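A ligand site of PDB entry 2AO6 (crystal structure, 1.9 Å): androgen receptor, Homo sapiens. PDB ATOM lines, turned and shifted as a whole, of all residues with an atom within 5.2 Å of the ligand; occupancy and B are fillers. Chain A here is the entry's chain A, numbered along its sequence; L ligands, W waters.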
ATOM      1  N   LEU A  31       4.811   3.308  -8.676  1.00  0.00           N
ATOM      2  CA  LEU A  31       3.603   4.085  -8.946  1.00  0.00           C
ATOM      3  C   LEU A  31       2.950   3.685 -10.272  1.00  0.00           C
ATOM      4  O   LEU A  31       1.718   3.675 -10.385  1.00  0.00           O
ATOM      5  CB  LEU A  31       3.913   5.576  -8.916  1.00  0.00           C
ATOM      6  CG  LEU A  31       4.221   6.110  -7.512  1.00  0.00           C
ATOM      7  CD1 LEU A  31       4.463   7.593  -7.593  1.00  0.00           C
ATOM      8  CD2 LEU A  31       3.055   5.840  -6.574  1.00  0.00           C
ATOM      9  N   LEU A  34       1.079   0.551  -9.512  1.00  0.00           N
ATOM     10  CA  LEU A  34      -0.131   0.841  -8.765  1.00  0.00           C
ATOM     11  C   LEU A  34      -1.211   1.378  -9.706  1.00  0.00           C
ATOM     12  O   LEU A  34      -2.360   0.944  -9.623  1.00  0.00           O
ATOM     13  CB  LEU A  34       0.145   1.862  -7.641  1.00  0.00           C
ATOM     14  CG  LEU A  34       0.812   1.291  -6.378  1.00  0.00           C
ATOM     15  CD1 LEU A  34       1.165   2.404  -5.410  1.00  0.00           C
ATOM     16  CD2 LEU A  34      -0.155   0.320  -5.705  1.00  0.00           C
ATOM     17  N   ASN A  35      -0.852   2.290 -10.606  1.00  0.00           N
ATOM     18  CA  ASN A  35      -1.814   2.852 -11.547  1.00  0.00           C
ATOM     19  C   ASN A  35      -2.410   1.788 -12.454  1.00  0.00           C
ATOM     20  O   ASN A  35      -3.605   1.796 -12.721  1.00  0.00           O
ATOM     21  CB  ASN A  35      -1.174   3.951 -12.408  1.00  0.00           C
ATOM     22  CG  ASN A  35      -0.966   5.240 -11.640  1.00  0.00           C
ATOM     23  OD1 ASN A  35      -1.616   5.480 -10.629  1.00  0.00           O
ATOM     24  ND2 ASN A  35      -0.051   6.083 -12.124  1.00  0.00           N
ATOM     25  N   LEU A  37      -2.658  -1.362 -11.739  1.00  0.00           N
ATOM     26  CA  LEU A  37      -3.488  -2.191 -10.881  1.00  0.00           C
ATOM     27  C   LEU A  37      -4.816  -1.467 -10.637  1.00  0.00           C
ATOM     28  O   LEU A  37      -5.874  -2.085 -10.596  1.00  0.00           O
ATOM     29  CB  LEU A  37      -2.785  -2.456  -9.541  1.00  0.00           C
ATOM     30  CG  LEU A  37      -3.597  -3.309  -8.547  1.00  0.00           C
ATOM     31  CD1 LEU A  37      -3.888  -4.677  -9.158  1.00  0.00           C
ATOM     32  CD2 LEU A  37      -2.827  -3.449  -7.248  1.00  0.00           C
ATOM     33  N   GLY A  38      -4.739  -0.150 -10.478  1.00  0.00           N
ATOM     34  CA  GLY A  38      -5.940   0.642 -10.247  1.00  0.00           C
ATOM     35  C   GLY A  38      -6.886   0.525 -11.422  1.00  0.00           C
ATOM     36  O   GLY A  38      -8.113   0.413 -11.257  1.00  0.00           O
ATOM     37  N   GLN A  41      -8.439  -2.900 -11.347  1.00  0.00           N
ATOM     38  CA  GLN A  41      -9.457  -2.990 -10.320  1.00  0.00           C
ATOM     39  C   GLN A  41     -10.692  -2.195 -10.687  1.00  0.00           C
ATOM     40  O   GLN A  41     -11.804  -2.598 -10.343  1.00  0.00           O
ATOM     41  CB  GLN A  41      -8.902  -2.520  -8.967  1.00  0.00           C
ATOM     42  CG  GLN A  41      -7.837  -3.468  -8.411  1.00  0.00           C
ATOM     43  CD  GLN A  41      -7.604  -3.292  -6.924  1.00  0.00           C
ATOM     44  OE1 GLN A  41      -6.743  -3.953  -6.331  1.00  0.00           O
ATOM     45  NE2 GLN A  41      -8.377  -2.403  -6.308  1.00  0.00           N
ATOM     46  N   TRP A  71     -14.751   4.878  -6.401  1.00  0.00           N
ATOM     47  CA  TRP A  71     -13.635   4.017  -6.775  1.00  0.00           C
ATOM     48  C   TRP A  71     -12.464   3.975  -5.781  1.00  0.00           C
ATOM     49  O   TRP A  71     -12.054   2.906  -5.336  1.00  0.00           O
ATOM     50  CB  TRP A  71     -13.166   4.421  -8.166  1.00  0.00           C
ATOM     51  CG  TRP A  71     -11.852   3.904  -8.605  1.00  0.00           C
ATOM     52  CD1 TRP A  71     -11.496   2.596  -8.793  1.00  0.00           C
ATOM     53  CD2 TRP A  71     -10.721   4.684  -8.982  1.00  0.00           C
ATOM     54  NE1 TRP A  71     -10.215   2.516  -9.270  1.00  0.00           N
ATOM     55  CE2 TRP A  71      -9.717   3.793  -9.397  1.00  0.00           C
ATOM     56  CE3 TRP A  71     -10.464   6.065  -9.010  1.00  0.00           C
ATOM     57  CZ2 TRP A  71      -8.474   4.228  -9.851  1.00  0.00           C
ATOM     58  CZ3 TRP A  71      -9.226   6.489  -9.456  1.00  0.00           C
ATOM     59  CH2 TRP A  71      -8.252   5.576  -9.871  1.00  0.00           C
ATOM     60  N   MET A  72     -11.931   5.139  -5.416  1.00  0.00           N
ATOM     61  CA  MET A  72     -10.804   5.180  -4.486  1.00  0.00           C
ATOM     62  C   MET A  72     -11.119   4.527  -3.140  1.00  0.00           C
ATOM     63  O   MET A  72     -10.347   3.684  -2.662  1.00  0.00           O
ATOM     64  CB  MET A  72     -10.358   6.624  -4.243  1.00  0.00           C
ATOM     65  CG  MET A  72      -9.063   6.729  -3.430  1.00  0.00           C
ATOM     66  SD  MET A  72      -7.617   6.082  -4.298  1.00  0.00           S
ATOM     67  CE  MET A  72      -7.322   7.435  -5.460  1.00  0.00           C
ATOM     68  N   MET A  75     -11.405   0.765  -3.359  1.00  0.00           N
ATOM     69  CA  MET A  75     -10.109   0.087  -3.460  1.00  0.00           C
ATOM     70  C   MET A  75      -9.377   0.063  -2.135  1.00  0.00           C
ATOM     71  O   MET A  75      -8.777  -0.947  -1.772  1.00  0.00           O
ATOM     72  CB  MET A  75      -9.220   0.774  -4.507  1.00  0.00           C
ATOM     73  CG  MET A  75      -9.747   0.685  -5.931  1.00  0.00           C
ATOM     74  SD  MET A  75      -8.462   1.114  -7.111  1.00  0.00           S
ATOM     75  CE  MET A  75      -8.112   2.801  -6.685  1.00  0.00           C
ATOM     76  N   VAL A  76      -9.438   1.171  -1.403  1.00  0.00           N
ATOM     77  CA  VAL A  76      -8.771   1.272  -0.110  1.00  0.00           C
ATOM     78  C   VAL A  76      -9.345   0.288   0.915  1.00  0.00           C
ATOM     79  O   VAL A  76      -8.607  -0.370   1.645  1.00  0.00           O
ATOM     80  CB  VAL A  76      -8.892   2.704   0.450  1.00  0.00           C
ATOM     81  CG1 VAL A  76      -8.365   2.762   1.870  1.00  0.00           C
ATOM     82  CG2 VAL A  76      -8.103   3.671  -0.432  1.00  0.00           C
ATOM     83  N   MET A  79      -8.524  -3.343  -0.097  1.00  0.00           N
ATOM     84  CA  MET A  79      -7.107  -3.575   0.103  1.00  0.00           C
ATOM     85  C   MET A  79      -6.819  -3.764   1.600  1.00  0.00           C
ATOM     86  O   MET A  79      -6.005  -4.594   1.996  1.00  0.00           O
ATOM     87  CB  MET A  79      -6.310  -2.396  -0.461  1.00  0.00           C
ATOM     88  CG  MET A  79      -4.811  -2.586  -0.494  1.00  0.00           C
ATOM     89  SD  MET A  79      -4.059  -2.299   1.111  1.00  0.00           S
ATOM     90  CE  MET A  79      -4.117  -0.497   1.183  1.00  0.00           C
ATOM     91  N   ARG A  82      -7.850  -7.253   2.437  1.00  0.00           N
ATOM     92  CA  ARG A  82      -6.885  -8.224   1.899  1.00  0.00           C
ATOM     93  C   ARG A  82      -5.631  -8.280   2.776  1.00  0.00           C
ATOM     94  O   ARG A  82      -5.077  -9.350   3.038  1.00  0.00           O
ATOM     95  CB  ARG A  82      -6.469  -7.859   0.480  1.00  0.00           C
ATOM     96  CG  ARG A  82      -7.455  -8.239  -0.604  1.00  0.00           C
ATOM     97  CD  ARG A  82      -6.754  -8.264  -1.960  1.00  0.00           C
ATOM     98  NE  ARG A  82      -6.200  -6.967  -2.330  1.00  0.00           N
ATOM     99  CZ  ARG A  82      -6.924  -5.944  -2.764  1.00  0.00           C
ATOM    100  NH1 ARG A  82      -8.250  -6.062  -2.881  1.00  0.00           N
ATOM    101  NH2 ARG A  82      -6.338  -4.804  -3.104  1.00  0.00           N
ATOM    102  N   TYR A  93      -1.225  -5.293   1.161  1.00  0.00           N
ATOM    103  CA  TYR A  93      -1.415  -6.281   0.103  1.00  0.00           C
ATOM    104  C   TYR A  93      -2.222  -5.676  -1.044  1.00  0.00           C
ATOM    105  O   TYR A  93      -3.400  -5.974  -1.210  1.00  0.00           O
ATOM    106  CB  TYR A  93      -2.149  -7.486   0.690  1.00  0.00           C
ATOM    107  CG  TYR A  93      -1.986  -8.794  -0.073  1.00  0.00           C
ATOM    108  CD1 TYR A  93      -1.019  -9.725   0.296  1.00  0.00           C
ATOM    109  CD2 TYR A  93      -2.837  -9.118  -1.127  1.00  0.00           C
ATOM    110  CE1 TYR A  93      -0.909 -10.950  -0.366  1.00  0.00           C
ATOM    111  CE2 TYR A  93      -2.745 -10.328  -1.781  1.00  0.00           C
ATOM    112  CZ  TYR A  93      -1.774 -11.241  -1.399  1.00  0.00           C
ATOM    113  OH  TYR A  93      -1.696 -12.458  -2.047  1.00  0.00           O
ATOM    114  N   PHE A  94      -1.589  -4.815  -1.832  1.00  0.00           N
ATOM    115  CA  PHE A  94      -2.292  -4.208  -2.953  1.00  0.00           C
ATOM    116  C   PHE A  94      -2.692  -5.328  -3.912  1.00  0.00           C
ATOM    117  O   PHE A  94      -3.803  -5.348  -4.443  1.00  0.00           O
ATOM    118  CB  PHE A  94      -1.378  -3.191  -3.654  1.00  0.00           C
ATOM    119  CG  PHE A  94      -1.165  -1.916  -2.877  1.00  0.00           C
ATOM    120  CD1 PHE A  94      -2.207  -1.002  -2.727  1.00  0.00           C
ATOM    121  CD2 PHE A  94       0.052  -1.643  -2.290  1.00  0.00           C
ATOM    122  CE1 PHE A  94      -2.030   0.171  -2.022  1.00  0.00           C
ATOM    123  CE2 PHE A  94       0.242  -0.456  -1.570  1.00  0.00           C
ATOM    124  CZ  PHE A  94      -0.801   0.442  -1.443  1.00  0.00           C
ATOM    125  N   MET A 110       4.463   7.795  -0.585  1.00  0.00           N
ATOM    126  CA  MET A 110       3.083   7.788  -0.101  1.00  0.00           C
ATOM    127  C   MET A 110       3.061   7.266   1.332  1.00  0.00           C
ATOM    128  O   MET A 110       2.032   6.768   1.789  1.00  0.00           O
ATOM    129  CB  MET A 110       2.200   6.845  -0.918  1.00  0.00           C
ATOM    130  CG  MET A 110       1.847   7.292  -2.306  1.00  0.00           C
ATOM    131  SD  MET A 110       0.430   6.314  -2.851  1.00  0.00           S
ATOM    132  CE  MET A 110       1.160   4.704  -2.923  1.00  0.00           C
ATOM    133  N   MET A 117      -3.599   3.598   5.809  1.00  0.00           N
ATOM    134  CA  MET A 117      -4.261   2.429   5.257  1.00  0.00           C
ATOM    135  C   MET A 117      -3.891   1.190   6.076  1.00  0.00           C
ATOM    136  O   MET A 117      -4.682   0.267   6.217  1.00  0.00           O
ATOM    137  CB  MET A 117      -3.876   2.224   3.781  1.00  0.00           C
ATOM    138  CG  MET A 117      -4.375   3.325   2.853  1.00  0.00           C
ATOM    139  SD  MET A 117      -4.099   3.024   1.080  1.00  0.00           S
ATOM    140  CE  MET A 117      -2.420   3.561   0.878  1.00  0.00           C
ATOM    141  N   LEU A 203      -5.572  10.273  -0.731  1.00  0.00           N
ATOM    142  CA  LEU A 203      -5.116   9.591  -1.938  1.00  0.00           C
ATOM    143  C   LEU A 203      -5.604  10.332  -3.177  1.00  0.00           C
ATOM    144  O   LEU A 203      -4.901  10.407  -4.179  1.00  0.00           O
ATOM    145  CB  LEU A 203      -5.632   8.150  -1.928  1.00  0.00           C
ATOM    146  CG  LEU A 203      -4.991   7.310  -0.829  1.00  0.00           C
ATOM    147  CD1 LEU A 203      -5.732   5.998  -0.703  1.00  0.00           C
ATOM    148  CD2 LEU A 203      -3.514   7.088  -1.141  1.00  0.00           C
ATOM    149  N   PHE A 206      -3.213  13.046  -3.634  1.00  0.00           N
ATOM    150  CA  PHE A 206      -1.936  12.511  -4.085  1.00  0.00           C
ATOM    151  C   PHE A 206      -1.947  12.119  -5.565  1.00  0.00           C
ATOM    152  O   PHE A 206      -1.052  12.516  -6.315  1.00  0.00           O
ATOM    153  CB  PHE A 206      -1.527  11.305  -3.232  1.00  0.00           C
ATOM    154  CG  PHE A 206      -0.189  10.720  -3.591  1.00  0.00           C
ATOM    155  CD1 PHE A 206      -0.069   9.792  -4.618  1.00  0.00           C
ATOM    156  CD2 PHE A 206       0.958  11.132  -2.931  1.00  0.00           C
ATOM    157  CE1 PHE A 206       1.169   9.285  -4.982  1.00  0.00           C
ATOM    158  CE2 PHE A 206       2.208  10.630  -3.291  1.00  0.00           C
ATOM    159  CZ  PHE A 206       2.310   9.709  -4.322  1.00  0.00           C
ATOM    160  N   THR A 207      -2.965  11.367  -5.987  1.00  0.00           N
ATOM    161  CA  THR A 207      -3.028  10.942  -7.380  1.00  0.00           C
ATOM    162  C   THR A 207      -3.254  12.141  -8.293  1.00  0.00           C
ATOM    163  O   THR A 207      -2.713  12.194  -9.399  1.00  0.00           O
ATOM    164  CB  THR A 207      -4.156   9.887  -7.606  1.00  0.00           C
ATOM    165  OG1 THR A 207      -3.904   9.179  -8.823  1.00  0.00           O
ATOM    166  CG2 THR A 207      -5.534  10.542  -7.683  1.00  0.00           C
ATOM    167  N   LEU A 210       0.066  13.799  -8.706  1.00  0.00           N
ATOM    168  CA  LEU A 210       0.904  12.903  -9.504  1.00  0.00           C
ATOM    169  C   LEU A 210       0.547  12.973 -10.991  1.00  0.00           C
ATOM    170  O   LEU A 210       1.436  12.954 -11.845  1.00  0.00           O
ATOM    171  CB  LEU A 210       0.778  11.463  -8.985  1.00  0.00           C
ATOM    172  CG  LEU A 210       1.645  10.376  -9.634  1.00  0.00           C
ATOM    173  CD1 LEU A 210       3.123  10.729  -9.502  1.00  0.00           C
ATOM    174  CD2 LEU A 210       1.376   9.039  -8.961  1.00  0.00           C
ATOM    175  N   PHE A 221      -0.143   6.763 -16.560  1.00  0.00           N
ATOM    176  CA  PHE A 221      -1.539   6.663 -16.122  1.00  0.00           C
ATOM    177  C   PHE A 221      -2.373   6.083 -17.266  1.00  0.00           C
ATOM    178  O   PHE A 221      -2.394   6.637 -18.363  1.00  0.00           O
ATOM    179  CB  PHE A 221      -2.112   8.032 -15.762  1.00  0.00           C
ATOM    180  CG  PHE A 221      -1.742   8.517 -14.380  1.00  0.00           C
ATOM    181  CD1 PHE A 221      -0.485   9.038 -14.126  1.00  0.00           C
ATOM    182  CD2 PHE A 221      -2.676   8.505 -13.354  1.00  0.00           C
ATOM    183  CE1 PHE A 221      -0.165   9.531 -12.859  1.00  0.00           C
ATOM    184  CE2 PHE A 221      -2.366   8.993 -12.100  1.00  0.00           C
ATOM    185  CZ  PHE A 221      -1.106   9.516 -11.856  1.00  0.00           C
ATOM    186  N   MET A 225      -8.246   5.941 -16.031  1.00  0.00           N
ATOM    187  CA  MET A 225      -7.858   6.599 -14.790  1.00  0.00           C
ATOM    188  C   MET A 225      -7.544   8.063 -15.001  1.00  0.00           C
ATOM    189  O   MET A 225      -8.056   8.919 -14.284  1.00  0.00           O
ATOM    190  CB  MET A 225      -6.628   5.909 -14.193  1.00  0.00           C
ATOM    191  CG  MET A 225      -6.928   4.666 -13.402  1.00  0.00           C
ATOM    192  SD  MET A 225      -5.425   4.095 -12.632  1.00  0.00           S
ATOM    193  CE  MET A 225      -5.105   5.410 -11.440  1.00  0.00           C
HETATM  194  C1  LIG L   1      -4.673   0.107  -6.369  1.00  0.00           C
HETATM  195  C2  LIG L   1      -5.717  -0.884  -5.841  1.00  0.00           C
HETATM  196  C3  LIG L   1      -5.626  -1.072  -4.340  1.00  0.00           C
HETATM  197  C4  LIG L   1      -5.538   0.160  -3.567  1.00  0.00           C
HETATM  198  C5  LIG L   1      -5.066   1.326  -4.108  1.00  0.00           C
HETATM  199  C6  LIG L   1      -5.021   2.592  -3.217  1.00  0.00           C
HETATM  200  C7  LIG L   1      -3.910   3.542  -3.660  1.00  0.00           C
HETATM  201  C8  LIG L   1      -4.120   3.932  -5.166  1.00  0.00           C
HETATM  202  C9  LIG L   1      -4.154   2.633  -6.069  1.00  0.00           C
HETATM  203  C10 LIG L   1      -4.601   1.433  -5.557  1.00  0.00           C
HETATM  204  C11 LIG L   1      -3.692   2.808  -7.479  1.00  0.00           C
HETATM  205  C12 LIG L   1      -3.254   3.981  -7.997  1.00  0.00           C
HETATM  206  C13 LIG L   1      -3.168   5.274  -7.154  1.00  0.00           C
HETATM  207  C14 LIG L   1      -3.009   4.868  -5.642  1.00  0.00           C
HETATM  208  C15 LIG L   1      -2.856   6.225  -4.901  1.00  0.00           C
HETATM  209  C16 LIG L   1      -2.135   7.082  -5.979  1.00  0.00           C
HETATM  210  C17 LIG L   1      -1.918   6.194  -7.257  1.00  0.00           C
HETATM  211  C18 LIG L   1      -4.511   6.057  -7.384  1.00  0.00           C
HETATM  212  C19 LIG L   1      -0.591   5.451  -7.141  1.00  0.00           C
HETATM  213  O1  LIG L   1      -5.662  -2.180  -3.801  1.00  0.00           O
HETATM  214  O2  LIG L   1      -1.924   7.045  -8.408  1.00  0.00           O
HETATM  215  O   HOH W   1      -8.757  -2.949  -3.587  1.00  0.00           O
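O2 of the ligand lies within hydrogen-bond range of OD1 of Asn 35. NH2 of Arg 82 sits at hydrogen-bond distance from O1 of the ligand (2.8 Å). An oxygen (O2) of the ligand is in hydrogen-bond range of the side-chain hydroxyl (OG1) of Thr 207, 2.9 Å away. OE1 of Gln 41 sits close to O1 of the ligand, at 3.3 Å.
The side-chain amide nitrogen of Asn 35 sits close to the backbone carbonyl oxygen of Leu 31, at 3.5 Å. The side-chain amide oxygen (OE1) of Gln 41 is in hydrogen-bond range of the guanidinium group (NH2) of Arg 82, at 3.4 Å. NH2 of Arg 82 lies within hydrogen-bond range of O of Phe 94 (2.9 Å). The backbone carbonyl oxygen (O) of Tyr 93 sits at hydrogen-bond distance from the guanidinium group (NE) of Arg 82 (3.2 Å). SD of Met 75 lies close to NE2 of Gln 41 (3.6 Å). NE1 of Trp 71 lies within hydrogen-bond range of SD of Met 75 (3.1 Å).
Residues that only touch the ligand: Leu 34, Met 79, Met 75, Phe 94, Phe 206, Met 72, Leu 31, Met 110, Leu 210 and Leu 203. 14 residues have an atom within 4 Å of the ligand: Leu 31, Leu 34, Asn 35, Gln 41, Met 72, Met 75, Met 79, Arg 82, Phe 94, Met 110, Leu 203, Phe 206, Thr 207 and Leu 210.
Water W1 lies within hydrogen-bond range of O of Met 75, NE2 of Gln 41, NH2 of Arg 82 and O1 of the ligand.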
